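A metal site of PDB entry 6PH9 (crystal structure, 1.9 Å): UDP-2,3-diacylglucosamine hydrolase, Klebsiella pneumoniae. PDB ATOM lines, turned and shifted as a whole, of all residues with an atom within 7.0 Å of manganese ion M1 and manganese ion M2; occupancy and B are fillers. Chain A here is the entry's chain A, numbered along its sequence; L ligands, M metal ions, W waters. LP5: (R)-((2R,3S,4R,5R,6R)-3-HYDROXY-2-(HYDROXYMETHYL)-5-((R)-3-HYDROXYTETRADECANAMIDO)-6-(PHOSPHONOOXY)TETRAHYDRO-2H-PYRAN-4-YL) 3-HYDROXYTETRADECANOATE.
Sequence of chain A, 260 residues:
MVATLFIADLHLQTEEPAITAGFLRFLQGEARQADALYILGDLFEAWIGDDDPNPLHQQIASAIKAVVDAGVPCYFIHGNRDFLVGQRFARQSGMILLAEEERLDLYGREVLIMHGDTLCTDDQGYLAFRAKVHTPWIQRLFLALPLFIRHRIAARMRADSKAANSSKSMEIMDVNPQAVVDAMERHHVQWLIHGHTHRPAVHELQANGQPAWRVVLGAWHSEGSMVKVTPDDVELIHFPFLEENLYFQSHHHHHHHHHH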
ATOM      1  N   ALA A   8       9.649  -9.867  -4.515  1.00  0.00           N
ATOM      2  CA  ALA A   8       8.910 -11.018  -5.008  1.00  0.00           C
ATOM      3  C   ALA A   8       7.935 -10.559  -6.076  1.00  0.00           C
ATOM      4  O   ALA A   8       7.653  -9.360  -6.206  1.00  0.00           O
ATOM      5  CB  ALA A   8       8.159 -11.735  -3.879  1.00  0.00           C
ATOM      6  N   ASP A   9       7.406 -11.527  -6.823  1.00  0.00           N
ATOM      7  CA  ASP A   9       6.311 -11.306  -7.763  1.00  0.00           C
ATOM      8  C   ASP A   9       6.653 -10.259  -8.816  1.00  0.00           C
ATOM      9  O   ASP A   9       5.843  -9.378  -9.138  1.00  0.00           O
ATOM     10  CB  ASP A   9       5.024 -10.940  -7.016  1.00  0.00           C
ATOM     11  CG  ASP A   9       4.574 -12.046  -6.077  1.00  0.00           C
ATOM     12  OD1 ASP A   9       4.190 -13.119  -6.567  1.00  0.00           O
ATOM     13  OD2 ASP A   9       4.642 -11.840  -4.840  1.00  0.00           O
ATOM     14  N   LEU A  10       7.869 -10.344  -9.367  1.00  0.00           N
ATOM     15  CA  LEU A  10       8.234  -9.493 -10.487  1.00  0.00           C
ATOM     16  C   LEU A  10       7.586  -9.966 -11.781  1.00  0.00           C
ATOM     17  O   LEU A  10       7.276  -9.147 -12.649  1.00  0.00           O
ATOM     18  CB  LEU A  10       9.758  -9.449 -10.625  1.00  0.00           C
ATOM     19  CG  LEU A  10      10.520  -8.731  -9.510  1.00  0.00           C
ATOM     20  CD1 LEU A  10      10.868  -9.690  -8.365  1.00  0.00           C
ATOM     21  CD2 LEU A  10      11.770  -8.091 -10.068  1.00  0.00           C
ATOM     22  N   HIS A  11       7.368 -11.279 -11.910  1.00  0.00           N
ATOM     23  CA  HIS A  11       6.717 -11.876 -13.077  1.00  0.00           C
ATOM     24  C   HIS A  11       7.355 -11.394 -14.372  1.00  0.00           C
ATOM     25  O   HIS A  11       6.686 -10.984 -15.325  1.00  0.00           O
ATOM     26  CB  HIS A  11       5.216 -11.582 -13.056  1.00  0.00           C
ATOM     27  CG  HIS A  11       4.459 -12.313 -11.983  1.00  0.00           C
ATOM     28  ND1 HIS A  11       3.843 -13.527 -12.212  1.00  0.00           N
ATOM     29  CD2 HIS A  11       4.221 -11.999 -10.689  1.00  0.00           C
ATOM     30  CE1 HIS A  11       3.256 -13.930 -11.097  1.00  0.00           C
ATOM     31  NE2 HIS A  11       3.474 -13.027 -10.158  1.00  0.00           N
ATOM     32  N   LEU A  40      11.618 -13.834  -3.068  1.00  0.00           N
ATOM     33  CA  LEU A  40      10.644 -14.770  -2.499  1.00  0.00           C
ATOM     34  C   LEU A  40       9.667 -15.319  -3.527  1.00  0.00           C
ATOM     35  O   LEU A  40       8.464 -15.404  -3.257  1.00  0.00           O
ATOM     36  CB  LEU A  40       9.903 -14.099  -1.349  1.00  0.00           C
ATOM     37  CG  LEU A  40      10.776 -13.553  -0.219  1.00  0.00           C
ATOM     38  CD1 LEU A  40       9.922 -13.109   0.960  1.00  0.00           C
ATOM     39  CD2 LEU A  40      11.796 -14.595   0.227  1.00  0.00           C
ATOM     40  N   GLY A  41      10.135 -15.700  -4.712  1.00  0.00           N
ATOM     41  CA  GLY A  41       9.289 -16.428  -5.636  1.00  0.00           C
ATOM     42  C   GLY A  41       8.650 -15.532  -6.685  1.00  0.00           C
ATOM     43  O   GLY A  41       8.488 -14.320  -6.513  1.00  0.00           O
ATOM     44  N   ASP A  42       8.237 -16.173  -7.781  1.00  0.00           N
ATOM     45  CA  ASP A  42       7.626 -15.485  -8.916  1.00  0.00           C
ATOM     46  C   ASP A  42       8.527 -14.384  -9.445  1.00  0.00           C
ATOM     47  O   ASP A  42       8.085 -13.276  -9.761  1.00  0.00           O
ATOM     48  CB  ASP A  42       6.240 -14.939  -8.559  1.00  0.00           C
ATOM     49  CG  ASP A  42       5.217 -16.045  -8.369  1.00  0.00           C
ATOM     50  OD1 ASP A  42       5.557 -17.217  -8.600  1.00  0.00           O
ATOM     51  OD2 ASP A  42       4.071 -15.725  -8.004  1.00  0.00           O
ATOM     52  N   GLY A  79       8.416 -19.714  -6.328  1.00  0.00           N
ATOM     53  CA  GLY A  79       7.026 -19.341  -6.373  1.00  0.00           C
ATOM     54  C   GLY A  79       6.205 -20.362  -7.151  1.00  0.00           C
ATOM     55  O   GLY A  79       6.714 -21.368  -7.638  1.00  0.00           O
ATOM     56  N   ASN A  80       4.913 -20.074  -7.266  1.00  0.00           N
ATOM     57  CA  ASN A  80       4.022 -20.943  -8.034  1.00  0.00           C
ATOM     58  C   ASN A  80       4.269 -20.819  -9.530  1.00  0.00           C
ATOM     59  O   ASN A  80       3.836 -21.704 -10.286  1.00  0.00           O
ATOM     60  CB  ASN A  80       2.570 -20.640  -7.702  1.00  0.00           C
ATOM     61  CG  ASN A  80       2.169 -19.223  -8.052  1.00  0.00           C
ATOM     62  OD1 ASN A  80       2.564 -18.275  -7.365  1.00  0.00           O
ATOM     63  ND2 ASN A  80       1.387 -19.065  -9.111  1.00  0.00           N
ATOM     64  N   ARG A  81       4.939 -19.762  -9.969  1.00  0.00           N
ATOM     65  CA  ARG A  81       5.251 -19.587 -11.388  1.00  0.00           C
ATOM     66  C   ARG A  81       6.584 -20.192 -11.788  1.00  0.00           C
ATOM     67  O   ARG A  81       6.740 -20.614 -12.937  1.00  0.00           O
ATOM     68  CB  ARG A  81       5.252 -18.104 -11.752  1.00  0.00           C
ATOM     69  CG  ARG A  81       3.922 -17.394 -11.547  1.00  0.00           C
ATOM     70  CD  ARG A  81       2.839 -17.966 -12.451  1.00  0.00           C
ATOM     71  NE  ARG A  81       1.612 -17.169 -12.361  1.00  0.00           N
ATOM     72  CZ  ARG A  81       1.410 -16.044 -13.032  1.00  0.00           C
ATOM     73  NH1 ARG A  81       2.345 -15.585 -13.845  1.00  0.00           N
ATOM     74  NH2 ARG A  81       0.272 -15.378 -12.890  1.00  0.00           N
ATOM     75  N   HIS A 115       7.097 -17.947  -0.051  1.00  0.00           N
ATOM     76  CA  HIS A 115       6.405 -17.287  -1.151  1.00  0.00           C
ATOM     77  C   HIS A 115       5.014 -16.841  -0.734  1.00  0.00           C
ATOM     78  O   HIS A 115       4.576 -15.731  -1.066  1.00  0.00           O
ATOM     79  CB  HIS A 115       6.319 -18.196  -2.364  1.00  0.00           C
ATOM     80  CG  HIS A 115       5.608 -17.556  -3.526  1.00  0.00           C
ATOM     81  ND1 HIS A 115       6.054 -16.395  -4.113  1.00  0.00           N
ATOM     82  CD2 HIS A 115       4.468 -17.897  -4.172  1.00  0.00           C
ATOM     83  CE1 HIS A 115       5.223 -16.051  -5.087  1.00  0.00           C
ATOM     84  NE2 HIS A 115       4.254 -16.950  -5.138  1.00  0.00           N
ATOM     85  N   GLY A 116       4.294 -17.689   0.013  1.00  0.00           N
ATOM     86  CA  GLY A 116       2.994 -17.347   0.556  1.00  0.00           C
ATOM     87  C   GLY A 116       1.848 -18.188   0.043  1.00  0.00           C
ATOM     88  O   GLY A 116       0.781 -18.196   0.679  1.00  0.00           O
ATOM     89  N   ASP A 117       2.012 -18.887  -1.073  1.00  0.00           N
ATOM     90  CA  ASP A 117       0.900 -19.654  -1.626  1.00  0.00           C
ATOM     91  C   ASP A 117       0.479 -20.793  -0.704  1.00  0.00           C
ATOM     92  O   ASP A 117      -0.702 -21.168  -0.682  1.00  0.00           O
ATOM     93  CB  ASP A 117       1.272 -20.213  -3.011  1.00  0.00           C
ATOM     94  CG  ASP A 117       2.516 -21.076  -2.965  1.00  0.00           C
ATOM     95  OD1 ASP A 117       3.581 -20.578  -2.547  1.00  0.00           O
ATOM     96  OD2 ASP A 117       2.424 -22.262  -3.359  1.00  0.00           O
ATOM     97  N   TYR A 126      -6.154 -25.540  -5.498  1.00  0.00           N
ATOM     98  CA  TYR A 126      -4.777 -25.119  -5.749  1.00  0.00           C
ATOM     99  C   TYR A 126      -3.786 -26.049  -5.077  1.00  0.00           C
ATOM    100  O   TYR A 126      -2.794 -26.456  -5.705  1.00  0.00           O
ATOM    101  CB  TYR A 126      -4.546 -23.686  -5.266  1.00  0.00           C
ATOM    102  CG  TYR A 126      -3.059 -23.379  -5.271  1.00  0.00           C
ATOM    103  CD1 TYR A 126      -2.374 -23.301  -6.472  1.00  0.00           C
ATOM    104  CD2 TYR A 126      -2.349 -23.247  -4.082  1.00  0.00           C
ATOM    105  CE1 TYR A 126      -1.015 -23.057  -6.495  1.00  0.00           C
ATOM    106  CE2 TYR A 126      -0.981 -23.003  -4.108  1.00  0.00           C
ATOM    107  CZ  TYR A 126      -0.320 -22.912  -5.316  1.00  0.00           C
ATOM    108  OH  TYR A 126       1.036 -22.661  -5.346  1.00  0.00           O
ATOM    109  N   GLY A 195       5.048 -13.122  -0.320  1.00  0.00           N
ATOM    110  CA  GLY A 195       4.473 -12.475  -1.481  1.00  0.00           C
ATOM    111  C   GLY A 195       3.224 -13.181  -1.959  1.00  0.00           C
ATOM    112  O   GLY A 195       2.326 -13.467  -1.158  1.00  0.00           O
ATOM    113  N   HIS A 196       3.145 -13.449  -3.275  1.00  0.00           N
ATOM    114  CA  HIS A 196       2.094 -14.217  -3.931  1.00  0.00           C
ATOM    115  C   HIS A 196       0.760 -13.470  -4.081  1.00  0.00           C
ATOM    116  O   HIS A 196       0.172 -13.470  -5.160  1.00  0.00           O
ATOM    117  CB  HIS A 196       1.830 -15.541  -3.211  1.00  0.00           C
ATOM    118  CG  HIS A 196       0.811 -16.398  -3.885  1.00  0.00           C
ATOM    119  ND1 HIS A 196       0.984 -16.901  -5.159  1.00  0.00           N
ATOM    120  CD2 HIS A 196      -0.411 -16.821  -3.484  1.00  0.00           C
ATOM    121  CE1 HIS A 196      -0.076 -17.600  -5.506  1.00  0.00           C
ATOM    122  NE2 HIS A 196      -0.942 -17.570  -4.512  1.00  0.00           N
ATOM    123  N   THR A 197       0.273 -12.853  -3.001  1.00  0.00           N
ATOM    124  CA  THR A 197      -1.088 -12.302  -3.047  1.00  0.00           C
ATOM    125  C   THR A 197      -1.157 -10.942  -3.745  1.00  0.00           C
ATOM    126  O   THR A 197      -2.262 -10.522  -4.130  1.00  0.00           O
ATOM    127  CB  THR A 197      -1.665 -12.173  -1.634  1.00  0.00           C
ATOM    128  OG1 THR A 197      -0.913 -11.206  -0.886  1.00  0.00           O
ATOM    129  CG2 THR A 197      -1.612 -13.507  -0.915  1.00  0.00           C
ATOM    130  N   HIS A 198      -0.032 -10.248  -3.904  1.00  0.00           N
ATOM    131  CA  HIS A 198       0.029  -8.958  -4.609  1.00  0.00           C
ATOM    132  C   HIS A 198      -0.778  -7.876  -3.889  1.00  0.00           C
ATOM    133  O   HIS A 198      -1.290  -6.955  -4.518  1.00  0.00           O
ATOM    134  CB  HIS A 198      -0.443  -9.076  -6.062  1.00  0.00           C
ATOM    135  CG  HIS A 198       0.327 -10.073  -6.874  1.00  0.00           C
ATOM    136  ND1 HIS A 198       0.160 -10.210  -8.242  1.00  0.00           N
ATOM    137  CD2 HIS A 198       1.266 -10.990  -6.519  1.00  0.00           C
ATOM    138  CE1 HIS A 198       0.952 -11.158  -8.688  1.00  0.00           C
ATOM    139  NE2 HIS A 198       1.639 -11.654  -7.667  1.00  0.00           N
ATOM    140  N   ALA A 219       3.472  -6.845  -6.150  1.00  0.00           N
ATOM    141  CA  ALA A 219       3.891  -7.225  -7.483  1.00  0.00           C
ATOM    142  C   ALA A 219       4.415  -6.006  -8.237  1.00  0.00           C
ATOM    143  O   ALA A 219       4.029  -4.867  -7.960  1.00  0.00           O
ATOM    144  CB  ALA A 219       2.739  -7.861  -8.260  1.00  0.00           C
HETATM  145  O48 LP5 L   1      -1.529 -16.119 -10.505  1.00  0.00           O
HETATM  146  P45 LP5 L   1      -1.908 -17.496 -11.007  1.00  0.00           P
HETATM  147  O46 LP5 L   1      -2.705 -17.369 -12.277  1.00  0.00           O
HETATM  148  O47 LP5 L   1      -0.653 -18.301 -11.270  1.00  0.00           O
HETATM  149  O1  LP5 L   1      -2.819 -18.259  -9.862  1.00  0.00           O
HETATM  150  C1  LP5 L   1      -2.190 -18.970  -8.867  1.00  0.00           C
HETATM  151  C2  LP5 L   1      -2.675 -20.414  -8.939  1.00  0.00           C
HETATM  152  N2  LP5 L   1      -2.375 -20.964 -10.285  1.00  0.00           N
HETATM  153  C7  LP5 L   1      -1.074 -21.562 -10.525  1.00  0.00           C
HETATM  154  C8  LP5 L   1      -0.751 -22.131 -11.901  1.00  0.00           C
HETATM  155  C16 LP5 L   1       0.404 -21.346 -12.494  1.00  0.00           C
HETATM  156  O44 LP5 L   1      -0.010 -20.045 -12.811  1.00  0.00           O
HETATM  157  C17 LP5 L   1       0.876 -22.044 -13.764  1.00  0.00           C
HETATM  158  C18 LP5 L   1       2.287 -21.535 -14.085  1.00  0.00           C
HETATM  159  C19 LP5 L   1       2.876 -22.393 -15.194  1.00  0.00           C
HETATM  160  C20 LP5 L   1       4.279 -22.838 -14.774  1.00  0.00           C
HETATM  161  C21 LP5 L   1       5.018 -23.351 -15.996  1.00  0.00           C
HETATM  162  C22 LP5 L   1       4.533 -24.768 -16.284  1.00  0.00           C
HETATM  163  C23 LP5 L   1       5.330 -25.722 -15.407  1.00  0.00           C
HETATM  164  C24 LP5 L   1       4.544 -27.013 -15.207  1.00  0.00           C
HETATM  165  C25 LP5 L   1       5.487 -28.076 -14.676  1.00  0.00           C
HETATM  166  C26 LP5 L   1       4.711 -29.342 -14.345  1.00  0.00           C
HETATM  167  C27 LP5 L   1       5.661 -30.358 -13.720  1.00  0.00           C
HETATM  168  O7  LP5 L   1      -0.269 -21.593  -9.659  1.00  0.00           O
HETATM  169  C3  LP5 L   1      -4.137 -20.514  -8.688  1.00  0.00           C
HETATM  170  C4  LP5 L   1      -4.526 -19.853  -7.431  1.00  0.00           C
HETATM  171  C5  LP5 L   1      -4.014 -18.414  -7.375  1.00  0.00           C
HETATM  172  O5  LP5 L   1      -2.530 -18.386  -7.575  1.00  0.00           O
HETATM  173  C6  LP5 L   1      -4.305 -17.850  -6.032  1.00  0.00           C
HETATM  174  O6  LP5 L   1      -3.534 -18.516  -5.077  1.00  0.00           O
HETATM  175  O4  LP5 L   1      -5.974 -19.827  -7.369  1.00  0.00           O
HETATM  176  O3  LP5 L   1      -4.491 -21.926  -8.580  1.00  0.00           O
HETATM  177  C28 LP5 L   1      -5.332 -22.396  -9.593  1.00  0.00           C
HETATM  178  O42 LP5 L   1      -6.063 -21.646 -10.151  1.00  0.00           O
HETATM  179  C29 LP5 L   1      -5.304 -23.873  -9.969  1.00  0.00           C
HETATM  180  C30 LP5 L   1      -6.727 -24.415 -10.075  1.00  0.00           C
HETATM  181  O43 LP5 L   1      -7.367 -24.342  -8.836  1.00  0.00           O
HETATM  182  C31 LP5 L   1      -6.636 -25.871 -10.546  1.00  0.00           C
HETATM  183  C32 LP5 L   1      -6.020 -25.870 -11.941  1.00  0.00           C
HETATM  184  C33 LP5 L   1      -5.488 -27.246 -12.304  1.00  0.00           C
HETATM  185  C34 LP5 L   1      -5.915 -27.575 -13.729  1.00  0.00           C
HETATM  186  C35 LP5 L   1      -4.777 -27.250 -14.691  1.00  0.00           C
HETATM  187  C36 LP5 L   1      -4.131 -28.553 -15.173  1.00  0.00           C
HETATM  188  C37 LP5 L   1      -3.667 -28.396 -16.614  1.00  0.00           C
HETATM  189  C38 LP5 L   1      -2.916 -29.652 -17.026  1.00  0.00           C
HETATM  190  C39 LP5 L   1      -2.695 -29.679 -18.536  1.00  0.00           C
HETATM  191  C40 LP5 L   1      -1.736 -30.810 -18.898  1.00  0.00           C
HETATM  192  C41 LP5 L   1      -1.449 -30.798 -20.392  1.00  0.00           C
HETATM  193 MN    MN M   1       2.718 -16.466  -6.563  1.00  0.00          MN
HETATM  194 MN    MN M   2       3.009 -13.407  -7.996  1.00  0.00          MN
HETATM  195  O   HOH W   1       1.740 -14.989  -7.274  1.00  0.00           O
HETATM  196  O   HOH W   2       0.876 -16.078  -9.348  1.00  0.00           O
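Water W2 lies within hydrogen-bond range of an oxygen (O48) of the ligand, the side-chain amide nitrogen of Asn 80 and the guanidinium group of Arg 81.
Manganese ion M1 is bound by water W1.
OD1 of Asn 80 is bound to manganese ion M1 (2.0 Å).
Manganese ion M1 is bound by OD2 of Asp 42 (2.1 Å).
Manganese ion M1 is bound by NE2 of His 115 (2.2 Å).
ND1 of His 196 binds manganese ion M1 (2.3 Å).
Manganese ion M1 has five donor atoms within binding distance.
Four residues have an atom within 4 Å of manganese ion M2: Asp 9, His 11, Asp 42 and His 198.
The nearest printed residue that does not touch manganese ion M2 is His 196 (4.01 Å).
Manganese ion M2 is bound by OD1 of Asp 9 (1.9 Å), water W1 (2.2 Å), NE2 of His 11 (2.2 Å), NE2 of His 198 (2.2 Å) and OD2 of Asp 42 (2.5 Å).
Manganese ion M2 has five donor atoms within binding distance.
OD2 of Asp 9 is in hydrogen-bond range of N of His 196 (2.7 Å).
N of Asp 9 sits at hydrogen-bond distance from O of Gly 41 (3.0 Å).
OD1 of Asp 42 sits at hydrogen-bond distance from N of Arg 81, at 3.0 Å.
N of Leu 10 sits at hydrogen-bond distance from O of Asp 42 (3.0 Å).
The backbone carbonyl oxygen (O) of His 115 lies within hydrogen-bond range of the backbone NH (N) of Gly 195.
A ring nitrogen (ND1) of His 115 is in hydrogen-bond range of the backbone carbonyl oxygen (O) of Leu 40, at 2.7 Å.
A ring nitrogen (ND1) of His 11 lies within hydrogen-bond range of the guanidinium group (NH1) of Arg 81.
NE2 of His 198 sits close to O of His 196.
O47 of the ligand sits at hydrogen-bond distance from ND2 of Asn 80, at 3.1 Å.
NE2 of His 196 lies within hydrogen-bond range of O6 of the ligand (2.8 Å).
O47 of the ligand is in salt-bridge range of NE of Arg 81, at 2.8 Å.
Within 4 Å of manganese ion M1: Asp 9, Asp 42, Asn 80, His 115 and His 196.
The nearest printed residue that does not touch manganese ion M1 is His 11 (5.0 Å).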
